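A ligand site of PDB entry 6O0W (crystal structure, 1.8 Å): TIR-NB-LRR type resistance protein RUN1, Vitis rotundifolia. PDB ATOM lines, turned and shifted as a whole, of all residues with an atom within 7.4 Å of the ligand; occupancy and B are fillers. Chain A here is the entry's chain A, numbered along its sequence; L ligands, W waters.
O2 of the ligand sits at hydrogen-bond distance from N of Glu 17. OE1 of Glu 17 is in hydrogen-bond range of O9 of the ligand (2.7 Å). The guanidinium group of Arg 15 lies within salt-bridge range of an oxygen (O2) of the ligand. The backbone carbonyl oxygen (O) of Gly 47 sits at hydrogen-bond distance from a nitrogen (N3) of the ligand, 2.7 Å away. The guanidinium group of Arg 20 is in salt-bridge range of an oxygen (O1) of the ligand (2.8 Å). An oxygen (O2) of the ligand sits at hydrogen-bond distance from the backbone NH of Gly 16. The indole nitrogen (NE1) of Trp 77 sits close to a nitrogen (N4) of the ligand (3.4 Å).
OE2 of Glu 17 lies within salt-bridge range of NH2 of Arg 15 (3.0 Å). The guanidinium group of Arg 15 is in hydrogen-bond range of the backbone carbonyl oxygen of Asn 71. The backbone carbonyl oxygen of Arg 15 sits at hydrogen-bond distance from the side-chain hydroxyl of Thr 19 (3.4 Å). O of Glu 48 sits at hydrogen-bond distance from NE1 of Trp 77. OG of Ser 75 lies close to N of Trp 77 (3.2 Å).
O of Arg 45 lies close to N4 of the ligand, 3.2 Å away. Arg 46 touches the ligand (C to N3, 3.2 Å). Eight residues have an atom within 4 Å of the ligand: Arg 15, Gly 16, Glu 17, Arg 20, Arg 45, Arg 46, Gly 47 and Trp 77. Along chain A the residues within 4 Å of the ligand span positions 15 to 77.
Water W2 lies within hydrogen-bond range of an oxygen (O1) of the ligand (2.7 Å) and the guanidinium group of Arg 20 (2.9 Å). Water W1 bridges an oxygen (O1) of the ligand (2.7 Å) and the guanidinium group of Arg 46 (3.1 Å). Water W4 lies within hydrogen-bond range of the side-chain hydroxyl of Ser 75 and an oxygen (O3) of the ligand.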
ATOM      1  N   PHE A  14     -19.767  -5.355  17.345  1.00  0.00           N
ATOM      2  CA  PHE A  14     -19.797  -6.583  18.130  1.00  0.00           C
ATOM      3  C   PHE A  14     -20.443  -6.295  19.472  1.00  0.00           C
ATOM      4  O   PHE A  14     -20.578  -5.127  19.896  1.00  0.00           O
ATOM      5  CB  PHE A  14     -18.378  -7.166  18.322  1.00  0.00           C
ATOM      6  CG  PHE A  14     -17.443  -6.256  19.084  1.00  0.00           C
ATOM      7  CD1 PHE A  14     -16.832  -5.187  18.452  1.00  0.00           C
ATOM      8  CD2 PHE A  14     -17.176  -6.488  20.426  1.00  0.00           C
ATOM      9  CE1 PHE A  14     -15.992  -4.328  19.145  1.00  0.00           C
ATOM     10  CE2 PHE A  14     -16.330  -5.618  21.148  1.00  0.00           C
ATOM     11  CZ  PHE A  14     -15.733  -4.550  20.499  1.00  0.00           C
ATOM     12  N   ARG A  15     -20.831  -7.369  20.168  1.00  0.00           N
ATOM     13  CA  ARG A  15     -21.350  -7.285  21.531  1.00  0.00           C
ATOM     14  C   ARG A  15     -20.231  -7.702  22.479  1.00  0.00           C
ATOM     15  O   ARG A  15     -19.841  -8.876  22.525  1.00  0.00           O
ATOM     16  CB  ARG A  15     -22.575  -8.182  21.705  1.00  0.00           C
ATOM     17  CG  ARG A  15     -23.120  -8.203  23.148  1.00  0.00           C
ATOM     18  CD  ARG A  15     -23.853  -6.903  23.499  1.00  0.00           C
ATOM     19  NE  ARG A  15     -23.782  -6.621  24.936  1.00  0.00           N
ATOM     20  CZ  ARG A  15     -24.719  -6.920  25.823  1.00  0.00           C
ATOM     21  NH1 ARG A  15     -25.850  -7.522  25.442  1.00  0.00           N
ATOM     22  NH2 ARG A  15     -24.538  -6.597  27.101  1.00  0.00           N
ATOM     23  N   GLY A  16     -19.706  -6.731  23.242  1.00  0.00           N
ATOM     24  CA  GLY A  16     -18.512  -7.011  24.021  1.00  0.00           C
ATOM     25  C   GLY A  16     -18.690  -8.149  25.013  1.00  0.00           C
ATOM     26  O   GLY A  16     -17.802  -9.010  25.144  1.00  0.00           O
ATOM     27  N   GLU A  17     -19.823  -8.184  25.699  1.00  0.00           N
ATOM     28  CA  GLU A  17     -20.033  -9.187  26.733  1.00  0.00           C
ATOM     29  C   GLU A  17     -19.968 -10.602  26.160  1.00  0.00           C
ATOM     30  O   GLU A  17     -19.635 -11.541  26.877  1.00  0.00           O
ATOM     31  CB  GLU A  17     -21.375  -8.976  27.436  1.00  0.00           C
ATOM     32  CG  GLU A  17     -21.232  -8.616  28.913  1.00  0.00           C
ATOM     33  CD  GLU A  17     -22.518  -8.063  29.505  1.00  0.00           C
ATOM     34  OE1 GLU A  17     -22.438  -7.103  30.308  1.00  0.00           O
ATOM     35  OE2 GLU A  17     -23.612  -8.573  29.163  1.00  0.00           O
ATOM     36  N   ASP A  18     -20.269 -10.748  24.873  1.00  0.00           N
ATOM     37  CA  ASP A  18     -20.144 -12.042  24.201  1.00  0.00           C
ATOM     38  C   ASP A  18     -18.736 -12.323  23.686  1.00  0.00           C
ATOM     39  O   ASP A  18     -18.212 -13.429  23.873  1.00  0.00           O
ATOM     40  CB  ASP A  18     -21.091 -12.129  23.008  1.00  0.00           C
ATOM     41  CG  ASP A  18     -22.557 -12.186  23.409  1.00  0.00           C
ATOM     42  OD1 ASP A  18     -22.862 -12.547  24.570  1.00  0.00           O
ATOM     43  OD2 ASP A  18     -23.396 -11.878  22.542  1.00  0.00           O
ATOM     44  N   THR A  19     -18.120 -11.366  22.975  1.00  0.00           N
ATOM     45  CA  THR A  19     -16.969 -11.689  22.140  1.00  0.00           C
ATOM     46  C   THR A  19     -15.756 -10.780  22.296  1.00  0.00           C
ATOM     47  O   THR A  19     -14.778 -10.969  21.564  1.00  0.00           O
ATOM     48  CB  THR A  19     -17.394 -11.685  20.651  1.00  0.00           C
ATOM     49  OG1 THR A  19     -17.835 -10.371  20.273  1.00  0.00           O
ATOM     50  CG2 THR A  19     -18.516 -12.690  20.365  1.00  0.00           C
ATOM     51  N   ARG A  20     -15.768  -9.830  23.242  1.00  0.00           N
ATOM     52  CA  ARG A  20     -14.695  -8.846  23.319  1.00  0.00           C
ATOM     53  C   ARG A  20     -13.327  -9.468  23.527  1.00  0.00           C
ATOM     54  O   ARG A  20     -12.350  -9.077  22.876  1.00  0.00           O
ATOM     55  CB  ARG A  20     -15.002  -7.850  24.457  1.00  0.00           C
ATOM     56  CG  ARG A  20     -13.827  -7.114  25.033  1.00  0.00           C
ATOM     57  CD  ARG A  20     -14.262  -6.422  26.329  1.00  0.00           C
ATOM     58  NE  ARG A  20     -15.299  -5.413  26.092  1.00  0.00           N
ATOM     59  CZ  ARG A  20     -16.508  -5.435  26.632  1.00  0.00           C
ATOM     60  NH1 ARG A  20     -16.864  -6.423  27.455  1.00  0.00           N
ATOM     61  NH2 ARG A  20     -17.381  -4.467  26.359  1.00  0.00           N
ATOM     62  N   LEU A  44     -14.303   2.083  27.631  1.00  0.00           N
ATOM     63  CA  LEU A  44     -15.492   1.800  28.425  1.00  0.00           C
ATOM     64  C   LEU A  44     -16.533   2.864  28.130  1.00  0.00           C
ATOM     65  O   LEU A  44     -16.300   4.051  28.397  1.00  0.00           O
ATOM     66  CB  LEU A  44     -15.156   1.764  29.908  1.00  0.00           C
ATOM     67  CG  LEU A  44     -16.292   1.421  30.864  1.00  0.00           C
ATOM     68  CD1 LEU A  44     -16.762  -0.009  30.639  1.00  0.00           C
ATOM     69  CD2 LEU A  44     -15.824   1.597  32.296  1.00  0.00           C
ATOM     70  N   ARG A  45     -17.683   2.464  27.596  1.00  0.00           N
ATOM     71  CA  ARG A  45     -18.720   3.388  27.160  1.00  0.00           C
ATOM     72  C   ARG A  45     -19.849   3.409  28.167  1.00  0.00           C
ATOM     73  O   ARG A  45     -20.519   2.390  28.368  1.00  0.00           O
ATOM     74  CB  ARG A  45     -19.247   2.976  25.790  1.00  0.00           C
ATOM     75  CG  ARG A  45     -18.171   2.876  24.732  1.00  0.00           C
ATOM     76  CD  ARG A  45     -17.572   4.255  24.473  1.00  0.00           C
ATOM     77  NE  ARG A  45     -16.580   4.209  23.407  1.00  0.00           N
ATOM     78  CZ  ARG A  45     -15.886   5.258  22.974  1.00  0.00           C
ATOM     79  NH1 ARG A  45     -16.065   6.456  23.539  1.00  0.00           N
ATOM     80  NH2 ARG A  45     -15.001   5.097  22.003  1.00  0.00           N
ATOM     81  N   ARG A  46     -20.122   4.579  28.753  1.00  0.00           N
ATOM     82  CA  ARG A  46     -21.253   4.697  29.675  1.00  0.00           C
ATOM     83  C   ARG A  46     -22.138   5.915  29.376  1.00  0.00           C
ATOM     84  O   ARG A  46     -22.965   6.271  30.218  1.00  0.00           O
ATOM     85  CB  ARG A  46     -20.772   4.705  31.122  1.00  0.00           C
ATOM     86  CG  ARG A  46     -20.420   3.304  31.660  1.00  0.00           C
ATOM     87  CD  ARG A  46     -21.553   2.292  31.373  1.00  0.00           C
ATOM     88  NE  ARG A  46     -21.263   0.945  31.849  1.00  0.00           N
ATOM     89  CZ  ARG A  46     -20.922  -0.087  31.071  1.00  0.00           C
ATOM     90  NH1 ARG A  46     -20.807   0.073  29.753  1.00  0.00           N
ATOM     91  NH2 ARG A  46     -20.683  -1.270  31.611  1.00  0.00           N
ATOM     92  N   GLY A  47     -22.018   6.530  28.198  1.00  0.00           N
ATOM     93  CA  GLY A  47     -22.937   7.596  27.854  1.00  0.00           C
ATOM     94  C   GLY A  47     -24.326   7.097  27.461  1.00  0.00           C
ATOM     95  O   GLY A  47     -24.505   5.961  27.023  1.00  0.00           O
ATOM     96  N   GLU A  48     -25.332   7.958  27.626  1.00  0.00           N
ATOM     97  CA  GLU A  48     -26.697   7.623  27.210  1.00  0.00           C
ATOM     98  C   GLU A  48     -26.745   7.161  25.764  1.00  0.00           C
ATOM     99  O   GLU A  48     -27.381   6.156  25.433  1.00  0.00           O
ATOM    100  CB  GLU A  48     -27.619   8.831  27.362  1.00  0.00           C
ATOM    101  CG  GLU A  48     -27.835   9.390  28.738  1.00  0.00           C
ATOM    102  CD  GLU A  48     -28.528  10.742  28.663  1.00  0.00           C
ATOM    103  OE1 GLU A  48     -29.540  10.938  29.358  1.00  0.00           O
ATOM    104  OE2 GLU A  48     -28.047  11.604  27.894  1.00  0.00           O
ATOM    105  N   ALA A  49     -26.104   7.925  24.878  1.00  0.00           N
ATOM    106  CA  ALA A  49     -26.150   7.683  23.441  1.00  0.00           C
ATOM    107  C   ALA A  49     -24.866   7.009  22.952  1.00  0.00           C
ATOM    108  O   ALA A  49     -23.900   6.831  23.688  1.00  0.00           O
ATOM    109  CB  ALA A  49     -26.388   8.995  22.689  1.00  0.00           C
ATOM    110  N   ILE A  50     -24.894   6.634  21.665  1.00  0.00           N
ATOM    111  CA  ILE A  50     -23.680   6.170  20.984  1.00  0.00           C
ATOM    112  C   ILE A  50     -22.635   7.270  20.968  1.00  0.00           C
ATOM    113  O   ILE A  50     -22.946   8.432  20.670  1.00  0.00           O
ATOM    114  CB  ILE A  50     -24.006   5.733  19.546  1.00  0.00           C
ATOM    115  CG1 ILE A  50     -24.912   4.498  19.548  1.00  0.00           C
ATOM    116  CG2 ILE A  50     -22.727   5.421  18.786  1.00  0.00           C
ATOM    117  CD1 ILE A  50     -24.156   3.209  19.678  1.00  0.00           C
ATOM    118  N   ALA A  51     -21.389   6.903  21.252  1.00  0.00           N
ATOM    119  CA  ALA A  51     -20.328   7.893  21.333  1.00  0.00           C
ATOM    120  C   ALA A  51     -20.092   8.532  19.964  1.00  0.00           C
ATOM    121  O   ALA A  51     -20.077   7.829  18.944  1.00  0.00           O
ATOM    122  CB  ALA A  51     -19.031   7.250  21.835  1.00  0.00           C
ATOM    123  N   LEU A  54     -17.606   6.821  17.737  1.00  0.00           N
ATOM    124  CA  LEU A  54     -18.037   5.630  17.011  1.00  0.00           C
ATOM    125  C   LEU A  54     -18.795   6.011  15.745  1.00  0.00           C
ATOM    126  O   LEU A  54     -18.543   5.451  14.666  1.00  0.00           O
ATOM    127  CB  LEU A  54     -18.920   4.756  17.901  1.00  0.00           C
ATOM    128  CG  LEU A  54     -18.302   4.120  19.157  1.00  0.00           C
ATOM    129  CD1 LEU A  54     -19.167   2.991  19.689  1.00  0.00           C
ATOM    130  CD2 LEU A  54     -16.914   3.631  18.874  1.00  0.00           C
ATOM    131  N   ASN A  71     -26.231 -12.397  22.303  1.00  0.00           N
ATOM    132  CA  ASN A  71     -26.800 -11.277  23.034  1.00  0.00           C
ATOM    133  C   ASN A  71     -26.614  -9.936  22.323  1.00  0.00           C
ATOM    134  O   ASN A  71     -26.780  -8.872  22.936  1.00  0.00           O
ATOM    135  CB  ASN A  71     -26.196 -11.229  24.435  1.00  0.00           C
ATOM    136  CG  ASN A  71     -26.567 -12.430  25.252  1.00  0.00           C
ATOM    137  OD1 ASN A  71     -27.740 -12.755  25.387  1.00  0.00           O
ATOM    138  ND2 ASN A  71     -25.565 -13.129  25.770  1.00  0.00           N
ATOM    139  N   ARG A  74     -29.578  -7.634  22.602  1.00  0.00           N
ATOM    140  CA  ARG A  74     -29.928  -7.190  23.944  1.00  0.00           C
ATOM    141  C   ARG A  74     -29.247  -5.881  24.326  1.00  0.00           C
ATOM    142  O   ARG A  74     -29.467  -5.401  25.436  1.00  0.00           O
ATOM    143  CB  ARG A  74     -29.553  -8.265  24.984  1.00  0.00           C
ATOM    144  CG  ARG A  74     -30.435  -9.493  24.952  1.00  0.00           C
ATOM    145  CD  ARG A  74     -30.072 -10.472  26.072  1.00  0.00           C
ATOM    146  NE  ARG A  74     -31.197 -11.350  26.371  1.00  0.00           N
ATOM    147  CZ  ARG A  74     -31.543 -12.396  25.637  1.00  0.00           C
ATOM    148  NH1 ARG A  74     -30.836 -12.705  24.548  1.00  0.00           N
ATOM    149  NH2 ARG A  74     -32.581 -13.139  25.972  1.00  0.00           N
ATOM    150  N   SER A  75     -28.413  -5.318  23.459  1.00  0.00           N
ATOM    151  CA  SER A  75     -27.797  -4.025  23.692  1.00  0.00           C
ATOM    152  C   SER A  75     -28.402  -2.999  22.731  1.00  0.00           C
ATOM    153  O   SER A  75     -28.274  -3.130  21.517  1.00  0.00           O
ATOM    154  CB  SER A  75     -26.274  -4.084  23.513  1.00  0.00           C
ATOM    155  OG  SER A  75     -25.741  -2.781  23.301  1.00  0.00           O
ATOM    156  N   ARG A  76     -29.060  -1.986  23.292  1.00  0.00           N
ATOM    157  CA  ARG A  76     -29.599  -0.939  22.449  1.00  0.00           C
ATOM    158  C   ARG A  76     -28.497  -0.163  21.738  1.00  0.00           C
ATOM    159  O   ARG A  76     -28.744   0.412  20.676  1.00  0.00           O
ATOM    160  CB  ARG A  76     -30.498  -0.001  23.256  1.00  0.00           C
ATOM    161  CG  ARG A  76     -29.813   0.803  24.368  1.00  0.00           C
ATOM    162  CD  ARG A  76     -30.889   1.593  25.109  1.00  0.00           C
ATOM    163  NE  ARG A  76     -30.385   2.449  26.194  1.00  0.00           N
ATOM    164  CZ  ARG A  76     -29.874   3.662  26.011  1.00  0.00           C
ATOM    165  NH1 ARG A  76     -29.784   4.174  24.783  1.00  0.00           N
ATOM    166  NH2 ARG A  76     -29.463   4.379  27.053  1.00  0.00           N
ATOM    167  N   TRP A  77     -27.276  -0.143  22.303  1.00  0.00           N
ATOM    168  CA  TRP A  77     -26.174   0.546  21.630  1.00  0.00           C
ATOM    169  C   TRP A  77     -25.679  -0.243  20.424  1.00  0.00           C
ATOM    170  O   TRP A  77     -25.397   0.359  19.380  1.00  0.00           O
ATOM    171  CB  TRP A  77     -25.047   0.806  22.634  1.00  0.00           C
ATOM    172  CG  TRP A  77     -25.503   1.677  23.780  1.00  0.00           C
ATOM    173  CD1 TRP A  77     -25.473   3.048  23.834  1.00  0.00           C
ATOM    174  CD2 TRP A  77     -26.078   1.239  25.008  1.00  0.00           C
ATOM    175  NE1 TRP A  77     -26.003   3.482  25.042  1.00  0.00           N
ATOM    176  CE2 TRP A  77     -26.382   2.386  25.772  1.00  0.00           C
ATOM    177  CE3 TRP A  77     -26.366  -0.029  25.538  1.00  0.00           C
ATOM    178  CZ2 TRP A  77     -26.942   2.315  27.045  1.00  0.00           C
ATOM    179  CZ3 TRP A  77     -26.944  -0.099  26.807  1.00  0.00           C
ATOM    180  CH2 TRP A  77     -27.216   1.071  27.538  1.00  0.00           C
ATOM    181  N   CYS A  78     -25.595  -1.580  20.518  1.00  0.00           N
ATOM    182  CA  CYS A  78     -25.281  -2.379  19.336  1.00  0.00           C
ATOM    183  C   CYS A  78     -26.330  -2.193  18.248  1.00  0.00           C
ATOM    184  O   CYS A  78     -26.008  -2.117  17.053  1.00  0.00           O
ATOM    185  CB  CYS A  78     -25.196  -3.857  19.687  1.00  0.00           C
ATOM    186  SG  CYS A  78     -23.736  -4.319  20.626  1.00  0.00           S
HETATM  187  P1  LIG L   1     -21.160  -4.521  26.570  1.00  0.00           P
HETATM  188  O1  LIG L   1     -19.973  -4.406  27.414  1.00  0.00           O
HETATM  189  O2  LIG L   1     -21.376  -5.859  25.882  1.00  0.00           O
HETATM  190  O3  LIG L   1     -21.222  -3.370  25.545  1.00  0.00           O
HETATM  191  P2  LIG L   1     -25.344  -2.572  33.244  1.00  0.00           P
HETATM  192  O4  LIG L   1     -24.627  -1.390  33.801  1.00  0.00           O
HETATM  193  O5  LIG L   1     -26.873  -2.359  33.135  1.00  0.00           O
HETATM  194  O6  LIG L   1     -25.073  -3.873  34.008  1.00  0.00           O
HETATM  195  O7  LIG L   1     -24.829  -2.793  31.716  1.00  0.00           O
HETATM  196  C1  LIG L   1     -24.998  -4.061  31.051  1.00  0.00           C
HETATM  197  C2  LIG L   1     -24.232  -4.028  29.743  1.00  0.00           C
HETATM  198  O8  LIG L   1     -24.898  -3.137  28.823  1.00  0.00           O
HETATM  199  C3  LIG L   1     -22.811  -3.498  29.833  1.00  0.00           C
HETATM  200  O9  LIG L   1     -21.876  -4.495  30.230  1.00  0.00           O
HETATM  201  C4  LIG L   1     -22.589  -3.102  28.383  1.00  0.00           C
HETATM  202  O10 LIG L   1     -22.439  -4.274  27.556  1.00  0.00           O
HETATM  203  C5  LIG L   1     -23.936  -2.495  28.014  1.00  0.00           C
HETATM  204  N1  LIG L   1     -24.003  -1.066  28.303  1.00  0.00           N
HETATM  205  C6  LIG L   1     -24.482  -0.476  29.436  1.00  0.00           C
HETATM  206  N2  LIG L   1     -24.454   0.830  29.424  1.00  0.00           N
HETATM  207  C7  LIG L   1     -23.901   1.133  28.187  1.00  0.00           C
HETATM  208  C8  LIG L   1     -23.596   2.351  27.558  1.00  0.00           C
HETATM  209  N3  LIG L   1     -23.857   3.552  28.092  1.00  0.00           N
HETATM  210  N4  LIG L   1     -23.036   2.300  26.323  1.00  0.00           N
HETATM  211  C9  LIG L   1     -22.819   1.104  25.773  1.00  0.00           C
HETATM  212  N5  LIG L   1     -23.079  -0.108  26.265  1.00  0.00           N
HETATM  213  C10 LIG L   1     -23.622  -0.026  27.485  1.00  0.00           C
HETATM  214  O   HOH W   1     -18.938  -2.194  28.666  1.00  0.00           O
HETATM  215  O   HOH W   2     -19.078  -6.164  29.269  1.00  0.00           O
HETATM  216  O   HOH W   3     -22.514   4.671  24.867  1.00  0.00           O
HETATM  217  O   HOH W   4     -23.483  -2.238  24.406  1.00  0.00           O
